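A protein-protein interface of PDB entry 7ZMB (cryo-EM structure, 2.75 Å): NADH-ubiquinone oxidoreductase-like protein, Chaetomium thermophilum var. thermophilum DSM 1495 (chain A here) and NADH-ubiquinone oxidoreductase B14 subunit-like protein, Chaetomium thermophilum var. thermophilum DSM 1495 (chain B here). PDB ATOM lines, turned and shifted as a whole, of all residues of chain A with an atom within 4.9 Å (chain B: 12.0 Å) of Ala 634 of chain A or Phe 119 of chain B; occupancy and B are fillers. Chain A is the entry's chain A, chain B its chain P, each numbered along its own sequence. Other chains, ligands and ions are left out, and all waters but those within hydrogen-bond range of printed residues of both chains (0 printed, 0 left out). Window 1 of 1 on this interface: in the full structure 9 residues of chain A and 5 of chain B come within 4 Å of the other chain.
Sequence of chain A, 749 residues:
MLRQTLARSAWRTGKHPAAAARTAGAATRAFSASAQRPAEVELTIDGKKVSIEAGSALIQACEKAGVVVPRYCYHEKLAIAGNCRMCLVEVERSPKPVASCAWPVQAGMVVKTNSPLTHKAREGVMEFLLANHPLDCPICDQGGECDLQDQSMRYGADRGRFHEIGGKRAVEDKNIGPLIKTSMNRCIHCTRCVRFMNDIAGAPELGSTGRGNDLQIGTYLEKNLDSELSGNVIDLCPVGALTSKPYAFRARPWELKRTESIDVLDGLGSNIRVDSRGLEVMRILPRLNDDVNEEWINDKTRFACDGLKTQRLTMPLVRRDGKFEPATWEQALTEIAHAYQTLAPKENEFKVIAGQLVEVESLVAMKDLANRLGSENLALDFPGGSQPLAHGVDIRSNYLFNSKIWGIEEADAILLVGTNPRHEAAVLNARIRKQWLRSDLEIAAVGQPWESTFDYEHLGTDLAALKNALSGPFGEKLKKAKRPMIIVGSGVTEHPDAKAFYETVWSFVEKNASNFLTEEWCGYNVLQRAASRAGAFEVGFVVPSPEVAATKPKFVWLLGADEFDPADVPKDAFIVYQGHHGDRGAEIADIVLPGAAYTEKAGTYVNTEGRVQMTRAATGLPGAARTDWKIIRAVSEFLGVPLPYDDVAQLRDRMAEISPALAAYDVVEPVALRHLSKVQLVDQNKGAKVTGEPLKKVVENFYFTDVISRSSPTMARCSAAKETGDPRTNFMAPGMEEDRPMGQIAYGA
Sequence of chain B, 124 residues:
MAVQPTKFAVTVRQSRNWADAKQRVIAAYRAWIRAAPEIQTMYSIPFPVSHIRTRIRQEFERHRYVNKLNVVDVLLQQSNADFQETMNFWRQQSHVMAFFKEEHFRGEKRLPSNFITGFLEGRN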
ATOM      1  N   TRP A 329      27.454  13.993 -12.326  1.00  0.00           N
ATOM      2  CA  TRP A 329      26.180  14.662 -12.084  1.00  0.00           C
ATOM      3  C   TRP A 329      25.401  14.869 -13.376  1.00  0.00           C
ATOM      4  O   TRP A 329      24.176  14.718 -13.397  1.00  0.00           O
ATOM      5  CB  TRP A 329      26.406  15.998 -11.382  1.00  0.00           C
ATOM      6  CG  TRP A 329      26.363  15.908  -9.898  1.00  0.00           C
ATOM      7  CD1 TRP A 329      27.421  15.985  -9.051  1.00  0.00           C
ATOM      8  CD2 TRP A 329      25.208  15.707  -9.082  1.00  0.00           C
ATOM      9  NE1 TRP A 329      27.002  15.852  -7.757  1.00  0.00           N
ATOM     10  CE2 TRP A 329      25.646  15.679  -7.745  1.00  0.00           C
ATOM     11  CE3 TRP A 329      23.848  15.544  -9.348  1.00  0.00           C
ATOM     12  CZ2 TRP A 329      24.774  15.497  -6.679  1.00  0.00           C
ATOM     13  CZ3 TRP A 329      22.985  15.375  -8.288  1.00  0.00           C
ATOM     14  CH2 TRP A 329      23.448  15.351  -6.970  1.00  0.00           C
ATOM     15  N   LEU A 333      21.641  13.218 -14.021  1.00  0.00           N
ATOM     16  CA  LEU A 333      20.446  13.997 -14.318  1.00  0.00           C
ATOM     17  C   LEU A 333      19.916  13.697 -15.714  1.00  0.00           C
ATOM     18  O   LEU A 333      18.701  13.702 -15.923  1.00  0.00           O
ATOM     19  CB  LEU A 333      20.733  15.487 -14.165  1.00  0.00           C
ATOM     20  CG  LEU A 333      21.033  16.003 -12.759  1.00  0.00           C
ATOM     21  CD1 LEU A 333      20.771  17.479 -12.698  1.00  0.00           C
ATOM     22  CD2 LEU A 333      20.219  15.268 -11.716  1.00  0.00           C
ATOM     23  N   ARG A 626      25.643  17.696  -3.184  1.00  0.00           N
ATOM     24  CA  ARG A 626      25.107  19.010  -3.474  1.00  0.00           C
ATOM     25  C   ARG A 626      24.108  19.390  -2.399  1.00  0.00           C
ATOM     26  O   ARG A 626      23.729  18.579  -1.556  1.00  0.00           O
ATOM     27  CB  ARG A 626      24.436  19.049  -4.851  1.00  0.00           C
ATOM     28  CG  ARG A 626      25.367  18.800  -5.990  1.00  0.00           C
ATOM     29  CD  ARG A 626      26.352  19.915  -6.165  1.00  0.00           C
ATOM     30  NE  ARG A 626      27.015  19.822  -7.457  1.00  0.00           N
ATOM     31  CZ  ARG A 626      28.143  19.158  -7.670  1.00  0.00           C
ATOM     32  NH1 ARG A 626      28.747  18.529  -6.670  1.00  0.00           N
ATOM     33  NH2 ARG A 626      28.666  19.132  -8.883  1.00  0.00           N
ATOM     34  N   LYS A 630      19.145  22.638  -4.588  1.00  0.00           N
ATOM     35  CA  LYS A 630      19.835  22.844  -5.853  1.00  0.00           C
ATOM     36  C   LYS A 630      19.718  21.625  -6.753  1.00  0.00           C
ATOM     37  O   LYS A 630      19.619  21.761  -7.975  1.00  0.00           O
ATOM     38  CB  LYS A 630      21.301  23.172  -5.612  1.00  0.00           C
ATOM     39  CG  LYS A 630      21.539  24.423  -4.829  1.00  0.00           C
ATOM     40  CD  LYS A 630      22.951  24.888  -5.033  1.00  0.00           C
ATOM     41  CE  LYS A 630      23.297  25.996  -4.074  1.00  0.00           C
ATOM     42  NZ  LYS A 630      22.594  25.833  -2.783  1.00  0.00           N
ATOM     43  N   ILE A 631      19.730  20.429  -6.167  1.00  0.00           N
ATOM     44  CA  ILE A 631      19.492  19.220  -6.946  1.00  0.00           C
ATOM     45  C   ILE A 631      18.112  19.274  -7.584  1.00  0.00           C
ATOM     46  O   ILE A 631      17.947  19.010  -8.779  1.00  0.00           O
ATOM     47  CB  ILE A 631      19.649  17.971  -6.064  1.00  0.00           C
ATOM     48  CG1 ILE A 631      21.092  17.812  -5.593  1.00  0.00           C
ATOM     49  CG2 ILE A 631      19.186  16.748  -6.812  1.00  0.00           C
ATOM     50  CD1 ILE A 631      21.236  17.012  -4.331  1.00  0.00           C
ATOM     51  N   ILE A 632      17.099  19.622  -6.790  1.00  0.00           N
ATOM     52  CA  ILE A 632      15.734  19.701  -7.300  1.00  0.00           C
ATOM     53  C   ILE A 632      15.632  20.784  -8.363  1.00  0.00           C
ATOM     54  O   ILE A 632      14.960  20.612  -9.386  1.00  0.00           O
ATOM     55  CB  ILE A 632      14.751  19.947  -6.141  1.00  0.00           C
ATOM     56  CG1 ILE A 632      14.881  18.850  -5.093  1.00  0.00           C
ATOM     57  CG2 ILE A 632      13.338  19.985  -6.647  1.00  0.00           C
ATOM     58  CD1 ILE A 632      14.099  19.104  -3.845  1.00  0.00           C
ATOM     59  N   ARG A 633      16.299  21.913  -8.139  1.00  0.00           N
ATOM     60  CA  ARG A 633      16.331  22.976  -9.134  1.00  0.00           C
ATOM     61  C   ARG A 633      17.129  22.561 -10.362  1.00  0.00           C
ATOM     62  O   ARG A 633      16.782  22.937 -11.486  1.00  0.00           O
ATOM     63  CB  ARG A 633      16.906  24.246  -8.517  1.00  0.00           C
ATOM     64  CG  ARG A 633      17.446  25.242  -9.518  1.00  0.00           C
ATOM     65  CD  ARG A 633      16.346  25.999 -10.244  1.00  0.00           C
ATOM     66  NE  ARG A 633      16.912  27.026 -11.103  1.00  0.00           N
ATOM     67  CZ  ARG A 633      17.340  26.819 -12.342  1.00  0.00           C
ATOM     68  NH1 ARG A 633      17.258  25.619 -12.889  1.00  0.00           N
ATOM     69  NH2 ARG A 633      17.852  27.821 -13.035  1.00  0.00           N
ATOM     70  N   ALA A 634      18.199  21.789 -10.170  1.00  0.00           N
ATOM     71  CA  ALA A 634      18.995  21.333 -11.307  1.00  0.00           C
ATOM     72  C   ALA A 634      18.203  20.398 -12.208  1.00  0.00           C
ATOM     73  O   ALA A 634      18.279  20.502 -13.436  1.00  0.00           O
ATOM     74  CB  ALA A 634      20.270  20.646 -10.823  1.00  0.00           C
ATOM     75  N   VAL A 635      17.447  19.468 -11.624  1.00  0.00           N
ATOM     76  CA  VAL A 635      16.714  18.526 -12.451  1.00  0.00           C
ATOM     77  C   VAL A 635      15.522  19.197 -13.125  1.00  0.00           C
ATOM     78  O   VAL A 635      15.077  18.740 -14.185  1.00  0.00           O
ATOM     79  CB  VAL A 635      16.282  17.303 -11.621  1.00  0.00           C
ATOM     80  CG1 VAL A 635      15.295  17.691 -10.553  1.00  0.00           C
ATOM     81  CG2 VAL A 635      15.742  16.216 -12.506  1.00  0.00           C
ATOM     82  N   SER A 636      15.010  20.292 -12.558  1.00  0.00           N
ATOM     83  CA  SER A 636      13.946  21.022 -13.232  1.00  0.00           C
ATOM     84  C   SER A 636      14.420  21.593 -14.565  1.00  0.00           C
ATOM     85  O   SER A 636      13.608  21.788 -15.473  1.00  0.00           O
ATOM     86  CB  SER A 636      13.394  22.126 -12.322  1.00  0.00           C
ATOM     87  OG  SER A 636      14.308  23.195 -12.152  1.00  0.00           O
ATOM     88  N   GLU A 637      15.719  21.861 -14.708  1.00  0.00           N
ATOM     89  CA  GLU A 637      16.262  22.175 -16.026  1.00  0.00           C
ATOM     90  C   GLU A 637      16.145  20.984 -16.966  1.00  0.00           C
ATOM     91  O   GLU A 637      15.643  21.112 -18.087  1.00  0.00           O
ATOM     92  CB  GLU A 637      17.726  22.609 -15.923  1.00  0.00           C
ATOM     93  CG  GLU A 637      17.944  24.101 -15.902  1.00  0.00           C
ATOM     94  CD  GLU A 637      17.430  24.782 -17.153  1.00  0.00           C
ATOM     95  OE1 GLU A 637      17.529  24.187 -18.248  1.00  0.00           O
ATOM     96  OE2 GLU A 637      16.916  25.916 -17.043  1.00  0.00           O
ATOM     97  N   PHE A 638      16.611  19.814 -16.526  1.00  0.00           N
ATOM     98  CA  PHE A 638      16.670  18.656 -17.410  1.00  0.00           C
ATOM     99  C   PHE A 638      15.283  18.160 -17.794  1.00  0.00           C
ATOM    100  O   PHE A 638      15.086  17.684 -18.915  1.00  0.00           O
ATOM    101  CB  PHE A 638      17.469  17.529 -16.755  1.00  0.00           C
ATOM    102  CG  PHE A 638      18.954  17.759 -16.745  1.00  0.00           C
ATOM    103  CD1 PHE A 638      19.508  18.766 -15.987  1.00  0.00           C
ATOM    104  CD2 PHE A 638      19.794  16.959 -17.490  1.00  0.00           C
ATOM    105  CE1 PHE A 638      20.864  18.973 -15.983  1.00  0.00           C
ATOM    106  CE2 PHE A 638      21.145  17.164 -17.487  1.00  0.00           C
ATOM    107  CZ  PHE A 638      21.680  18.168 -16.731  1.00  0.00           C
ATOM    108  N   LEU B 111      33.369  33.167 -13.034  1.00  0.00           N
ATOM    109  CA  LEU B 111      32.087  32.768 -12.465  1.00  0.00           C
ATOM    110  C   LEU B 111      31.196  32.137 -13.528  1.00  0.00           C
ATOM    111  O   LEU B 111      31.184  32.587 -14.673  1.00  0.00           O
ATOM    112  CB  LEU B 111      31.387  33.970 -11.829  1.00  0.00           C
ATOM    113  CG  LEU B 111      32.075  34.558 -10.596  1.00  0.00           C
ATOM    114  CD1 LEU B 111      31.395  35.843 -10.164  1.00  0.00           C
ATOM    115  CD2 LEU B 111      32.093  33.547  -9.456  1.00  0.00           C
ATOM    116  N   PRO B 112      30.461  31.090 -13.152  1.00  0.00           N
ATOM    117  CA  PRO B 112      29.595  30.412 -14.123  1.00  0.00           C
ATOM    118  C   PRO B 112      28.537  31.355 -14.676  1.00  0.00           C
ATOM    119  O   PRO B 112      28.007  32.208 -13.963  1.00  0.00           O
ATOM    120  CB  PRO B 112      28.968  29.272 -13.310  1.00  0.00           C
ATOM    121  CG  PRO B 112      29.122  29.674 -11.885  1.00  0.00           C
ATOM    122  CD  PRO B 112      30.382  30.480 -11.815  1.00  0.00           C
ATOM    123  N   SER B 113      28.237  31.194 -15.963  1.00  0.00           N
ATOM    124  CA  SER B 113      27.295  32.074 -16.642  1.00  0.00           C
ATOM    125  C   SER B 113      25.842  31.694 -16.394  1.00  0.00           C
ATOM    126  O   SER B 113      24.949  32.471 -16.743  1.00  0.00           O
ATOM    127  CB  SER B 113      27.576  32.079 -18.147  1.00  0.00           C
ATOM    128  OG  SER B 113      26.866  33.120 -18.796  1.00  0.00           O
ATOM    129  N   ASN B 114      25.590  30.531 -15.800  1.00  0.00           N
ATOM    130  CA  ASN B 114      24.244  30.060 -15.516  1.00  0.00           C
ATOM    131  C   ASN B 114      24.267  29.267 -14.221  1.00  0.00           C
ATOM    132  O   ASN B 114      25.323  28.834 -13.757  1.00  0.00           O
ATOM    133  CB  ASN B 114      23.696  29.191 -16.648  1.00  0.00           C
ATOM    134  CG  ASN B 114      23.304  29.998 -17.861  1.00  0.00           C
ATOM    135  OD1 ASN B 114      23.958  29.936 -18.903  1.00  0.00           O
ATOM    136  ND2 ASN B 114      22.225  30.761 -17.739  1.00  0.00           N
ATOM    137  N   PHE B 115      23.086  29.089 -13.630  1.00  0.00           N
ATOM    138  CA  PHE B 115      22.981  28.228 -12.460  1.00  0.00           C
ATOM    139  C   PHE B 115      23.359  26.799 -12.812  1.00  0.00           C
ATOM    140  O   PHE B 115      24.091  26.138 -12.069  1.00  0.00           O
ATOM    141  CB  PHE B 115      21.564  28.274 -11.878  1.00  0.00           C
ATOM    142  CG  PHE B 115      21.303  27.205 -10.856  1.00  0.00           C
ATOM    143  CD1 PHE B 115      20.915  25.930 -11.241  1.00  0.00           C
ATOM    144  CD2 PHE B 115      21.466  27.467  -9.507  1.00  0.00           C
ATOM    145  CE1 PHE B 115      20.712  24.943 -10.307  1.00  0.00           C
ATOM    146  CE2 PHE B 115      21.247  26.474  -8.569  1.00  0.00           C
ATOM    147  CZ  PHE B 115      20.873  25.216  -8.973  1.00  0.00           C
ATOM    148  N   ILE B 116      22.854  26.300 -13.938  1.00  0.00           N
ATOM    149  CA  ILE B 116      23.039  24.896 -14.274  1.00  0.00           C
ATOM    150  C   ILE B 116      24.498  24.616 -14.598  1.00  0.00           C
ATOM    151  O   ILE B 116      25.028  23.554 -14.256  1.00  0.00           O
ATOM    152  CB  ILE B 116      22.089  24.492 -15.420  1.00  0.00           C
ATOM    153  CG1 ILE B 116      22.330  23.047 -15.865  1.00  0.00           C
ATOM    154  CG2 ILE B 116      22.218  25.437 -16.586  1.00  0.00           C
ATOM    155  CD1 ILE B 116      22.031  22.021 -14.809  1.00  0.00           C
ATOM    156  N   THR B 117      25.174  25.560 -15.256  1.00  0.00           N
ATOM    157  CA  THR B 117      26.607  25.414 -15.488  1.00  0.00           C
ATOM    158  C   THR B 117      27.370  25.398 -14.173  1.00  0.00           C
ATOM    159  O   THR B 117      28.268  24.575 -13.972  1.00  0.00           O
ATOM    160  CB  THR B 117      27.121  26.535 -16.386  1.00  0.00           C
ATOM    161  OG1 THR B 117      26.442  26.492 -17.645  1.00  0.00           O
ATOM    162  CG2 THR B 117      28.604  26.386 -16.627  1.00  0.00           C
ATOM    163  N   GLY B 118      27.014  26.299 -13.261  1.00  0.00           N
ATOM    164  CA  GLY B 118      27.641  26.297 -11.951  1.00  0.00           C
ATOM    165  C   GLY B 118      27.361  25.031 -11.169  1.00  0.00           C
ATOM    166  O   GLY B 118      28.238  24.513 -10.484  1.00  0.00           O
ATOM    167  N   PHE B 119      26.137  24.516 -11.261  1.00  0.00           N
ATOM    168  CA  PHE B 119      25.785  23.332 -10.485  1.00  0.00           C
ATOM    169  C   PHE B 119      26.593  22.124 -10.923  1.00  0.00           C
ATOM    170  O   PHE B 119      27.048  21.339 -10.088  1.00  0.00           O
ATOM    171  CB  PHE B 119      24.291  23.035 -10.613  1.00  0.00           C
ATOM    172  CG  PHE B 119      23.875  21.747  -9.964  1.00  0.00           C
ATOM    173  CD1 PHE B 119      23.548  21.707  -8.621  1.00  0.00           C
ATOM    174  CD2 PHE B 119      23.812  20.576 -10.695  1.00  0.00           C
ATOM    175  CE1 PHE B 119      23.164  20.522  -8.028  1.00  0.00           C
ATOM    176  CE2 PHE B 119      23.439  19.393 -10.097  1.00  0.00           C
ATOM    177  CZ  PHE B 119      23.108  19.367  -8.767  1.00  0.00           C
ATOM    178  N   LEU B 120      26.774  21.956 -12.230  1.00  0.00           N
ATOM    179  CA  LEU B 120      27.305  20.706 -12.755  1.00  0.00           C
ATOM    180  C   LEU B 120      28.802  20.575 -12.526  1.00  0.00           C
ATOM    181  O   LEU B 120      29.321  19.456 -12.478  1.00  0.00           O
ATOM    182  CB  LEU B 120      26.979  20.595 -14.240  1.00  0.00           C
ATOM    183  CG  LEU B 120      25.534  20.240 -14.573  1.00  0.00           C
ATOM    184  CD1 LEU B 120      25.376  20.036 -16.062  1.00  0.00           C
ATOM    185  CD2 LEU B 120      25.080  19.005 -13.812  1.00  0.00           C
ATOM    186  N   GLU B 121      29.511  21.685 -12.384  1.00  0.00           N
ATOM    187  CA  GLU B 121      30.952  21.660 -12.200  1.00  0.00           C
ATOM    188  C   GLU B 121      31.376  21.717 -10.738  1.00  0.00           C
ATOM    189  O   GLU B 121      32.571  21.844 -10.464  1.00  0.00           O
ATOM    190  CB  GLU B 121      31.592  22.824 -12.960  1.00  0.00           C
ATOM    191  CG  GLU B 121      31.486  22.726 -14.466  1.00  0.00           C
ATOM    192  CD  GLU B 121      32.118  23.906 -15.182  1.00  0.00           C
ATOM    193  OE1 GLU B 121      32.531  24.866 -14.500  1.00  0.00           O
ATOM    194  OE2 GLU B 121      32.207  23.870 -16.426  1.00  0.00           O
ATOM    195  N   GLY B 122      30.445  21.615  -9.802  1.00  0.00           N
ATOM    196  CA  GLY B 122      30.654  22.160  -8.479  1.00  0.00           C
ATOM    197  C   GLY B 122      30.520  23.669  -8.516  1.00  0.00           C
ATOM    198  O   GLY B 122      30.596  24.295  -9.566  1.00  0.00           O
ATOM    199  N   ARG B 123      30.299  24.267  -7.344  1.00  0.00           N
ATOM    200  CA  ARG B 123      29.982  25.693  -7.306  1.00  0.00           C
ATOM    201  C   ARG B 123      31.036  26.473  -8.070  1.00  0.00           C
ATOM    202  O   ARG B 123      32.186  26.562  -7.639  1.00  0.00           O
ATOM    203  CB  ARG B 123      29.902  26.193  -5.867  1.00  0.00           C
ATOM    204  CG  ARG B 123      29.363  27.598  -5.764  1.00  0.00           C
ATOM    205  CD  ARG B 123      29.246  28.056  -4.337  1.00  0.00           C
ATOM    206  NE  ARG B 123      30.537  28.401  -3.752  1.00  0.00           N
ATOM    207  CZ  ARG B 123      31.204  27.634  -2.900  1.00  0.00           C
ATOM    208  NH1 ARG B 123      30.716  26.462  -2.525  1.00  0.00           N
ATOM    209  NH2 ARG B 123      32.368  28.043  -2.427  1.00  0.00           N
ATOM    210  N   ASN B 124      30.633  27.033  -9.205  1.00  0.00           N
ATOM    211  CA  ASN B 124      31.567  27.413 -10.263  1.00  0.00           C
ATOM    212  C   ASN B 124      32.348  26.187 -10.722  1.00  0.00           C
ATOM    213  O   ASN B 124      33.203  25.661 -10.012  1.00  0.00           O
ATOM    214  CB  ASN B 124      32.531  28.512  -9.812  1.00  0.00           C
ATOM    215  CG  ASN B 124      33.515  28.888 -10.881  1.00  0.00           C
ATOM    216  OD1 ASN B 124      33.333  28.564 -12.052  1.00  0.00           O
ATOM    217  ND2 ASN B 124      34.562  29.589 -10.492  1.00  0.00           N
ATOM    218  OXT ASN B 124      32.133  25.689 -11.825  1.00  0.00           O
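Of the 14 printed residues of chain B, 5 touch a printed residue of chain A. Hydrophobic or aromatic side chains of chain B within 4 Å of the printed part of chain A: Phe 115, Ile 116 and Phe 119. Along chain B the printed residues that touch a printed residue of chain A span positions 115 to 122. Of the 12 printed residues of chain A, 7 touch a printed residue of chain B. Printed residues of chain A that touch a printed residue of chain B: Trp 329, Arg 626, Lys 630, Ile 631, Arg 633, Ala 634 and Phe 638. Hydrophobic or aromatic side chains of chain A within 4 Å of the printed part of chain B: Trp 329, Ala 634 and Phe 638. Among the printed residues, 10 pairs touch across the chains. Among the printed residues, no Asp or Glu carboxylate lies within 4 Å of a Lys or Arg side-chain nitrogen of the other chain.
Of the printed residues of chain A, Phe 119 of chain B touches Trp 329, Arg 626, Lys 630, Ile 631 and Ala 634. Of chain B, only Phe 119 (3.9 Å) comes within 4 Å of Trp 329 of chain A. Arg 626 of chain A touches three residues of chain B. Printed residues of chain B within 4 Å of Lys 630 of chain A: Phe 115 (3.8 Å) and Phe 119 (3.8 Å). Of the printed residues of chain B, Ile 631 of chain A touches Phe 119. Arg 633 of chain A touches just one residue of chain B: Phe 115 (3.4 Å). No residue of chain B comes within 4 Å of Val 635 of chain A. No residue of chain B comes within 4 Å of Ser 636 of chain A. No residue of chain B comes within 4 Å of Glu 637 of chain A. Printed residues of chain A within 4 Å of Phe 115 of chain B: Lys 630 and Arg 633. Of the printed residues of chain A, Ile 116 of chain B touches Phe 638. Printed residues of chain A within 4 Å of Leu 120 of chain B: Arg 626 (3.7 Å). Printed residues of chain A within 4 Å of Gly 122 of chain B: Arg 626 (3.2 Å). The nearest residue of chain A that does not touch Phe 119 of chain B is Leu 333 of chain A (4.2 Å). The nearest printed residue of chain A that does not touch Phe 115 of chain B is Ala 634 of chain A (4.04 Å).
Trp 329 of chain A touches Phe 119 of chain B (CE3 to CZ, 3.9 Å). O of Leu 120 of chain B touches NH2 of Arg 626 of chain A, 3.7 Å away. CZ of Phe 115 of chain B touches O of Lys 630 of chain A, at 3.8 Å. Lys 630 of chain A touches Phe 119 of chain B. Phe 119 of chain B touches Ile 631 of chain A. CE1 of Phe 115 of chain B touches CG of Arg 633 of chain A (3.4 Å). CB of Ala 634 of chain A touches CE2 of Phe 119 of chain B, 3.5 Å away. Ile 116 of chain B touches Phe 638 of chain A.
OG of Ser 636 of chain A lies within hydrogen-bond range of O of Arg 633 of chain A, 2.6 Å away.
The backbone carbonyl oxygen (O) of Phe 119 of chain B sits at hydrogen-bond distance from the guanidinium group (NH2) of Arg 626 of chain A (3.0 Å). N of Gly 122 of chain B lies close to NH2 of Arg 626 of chain A (3.2 Å).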
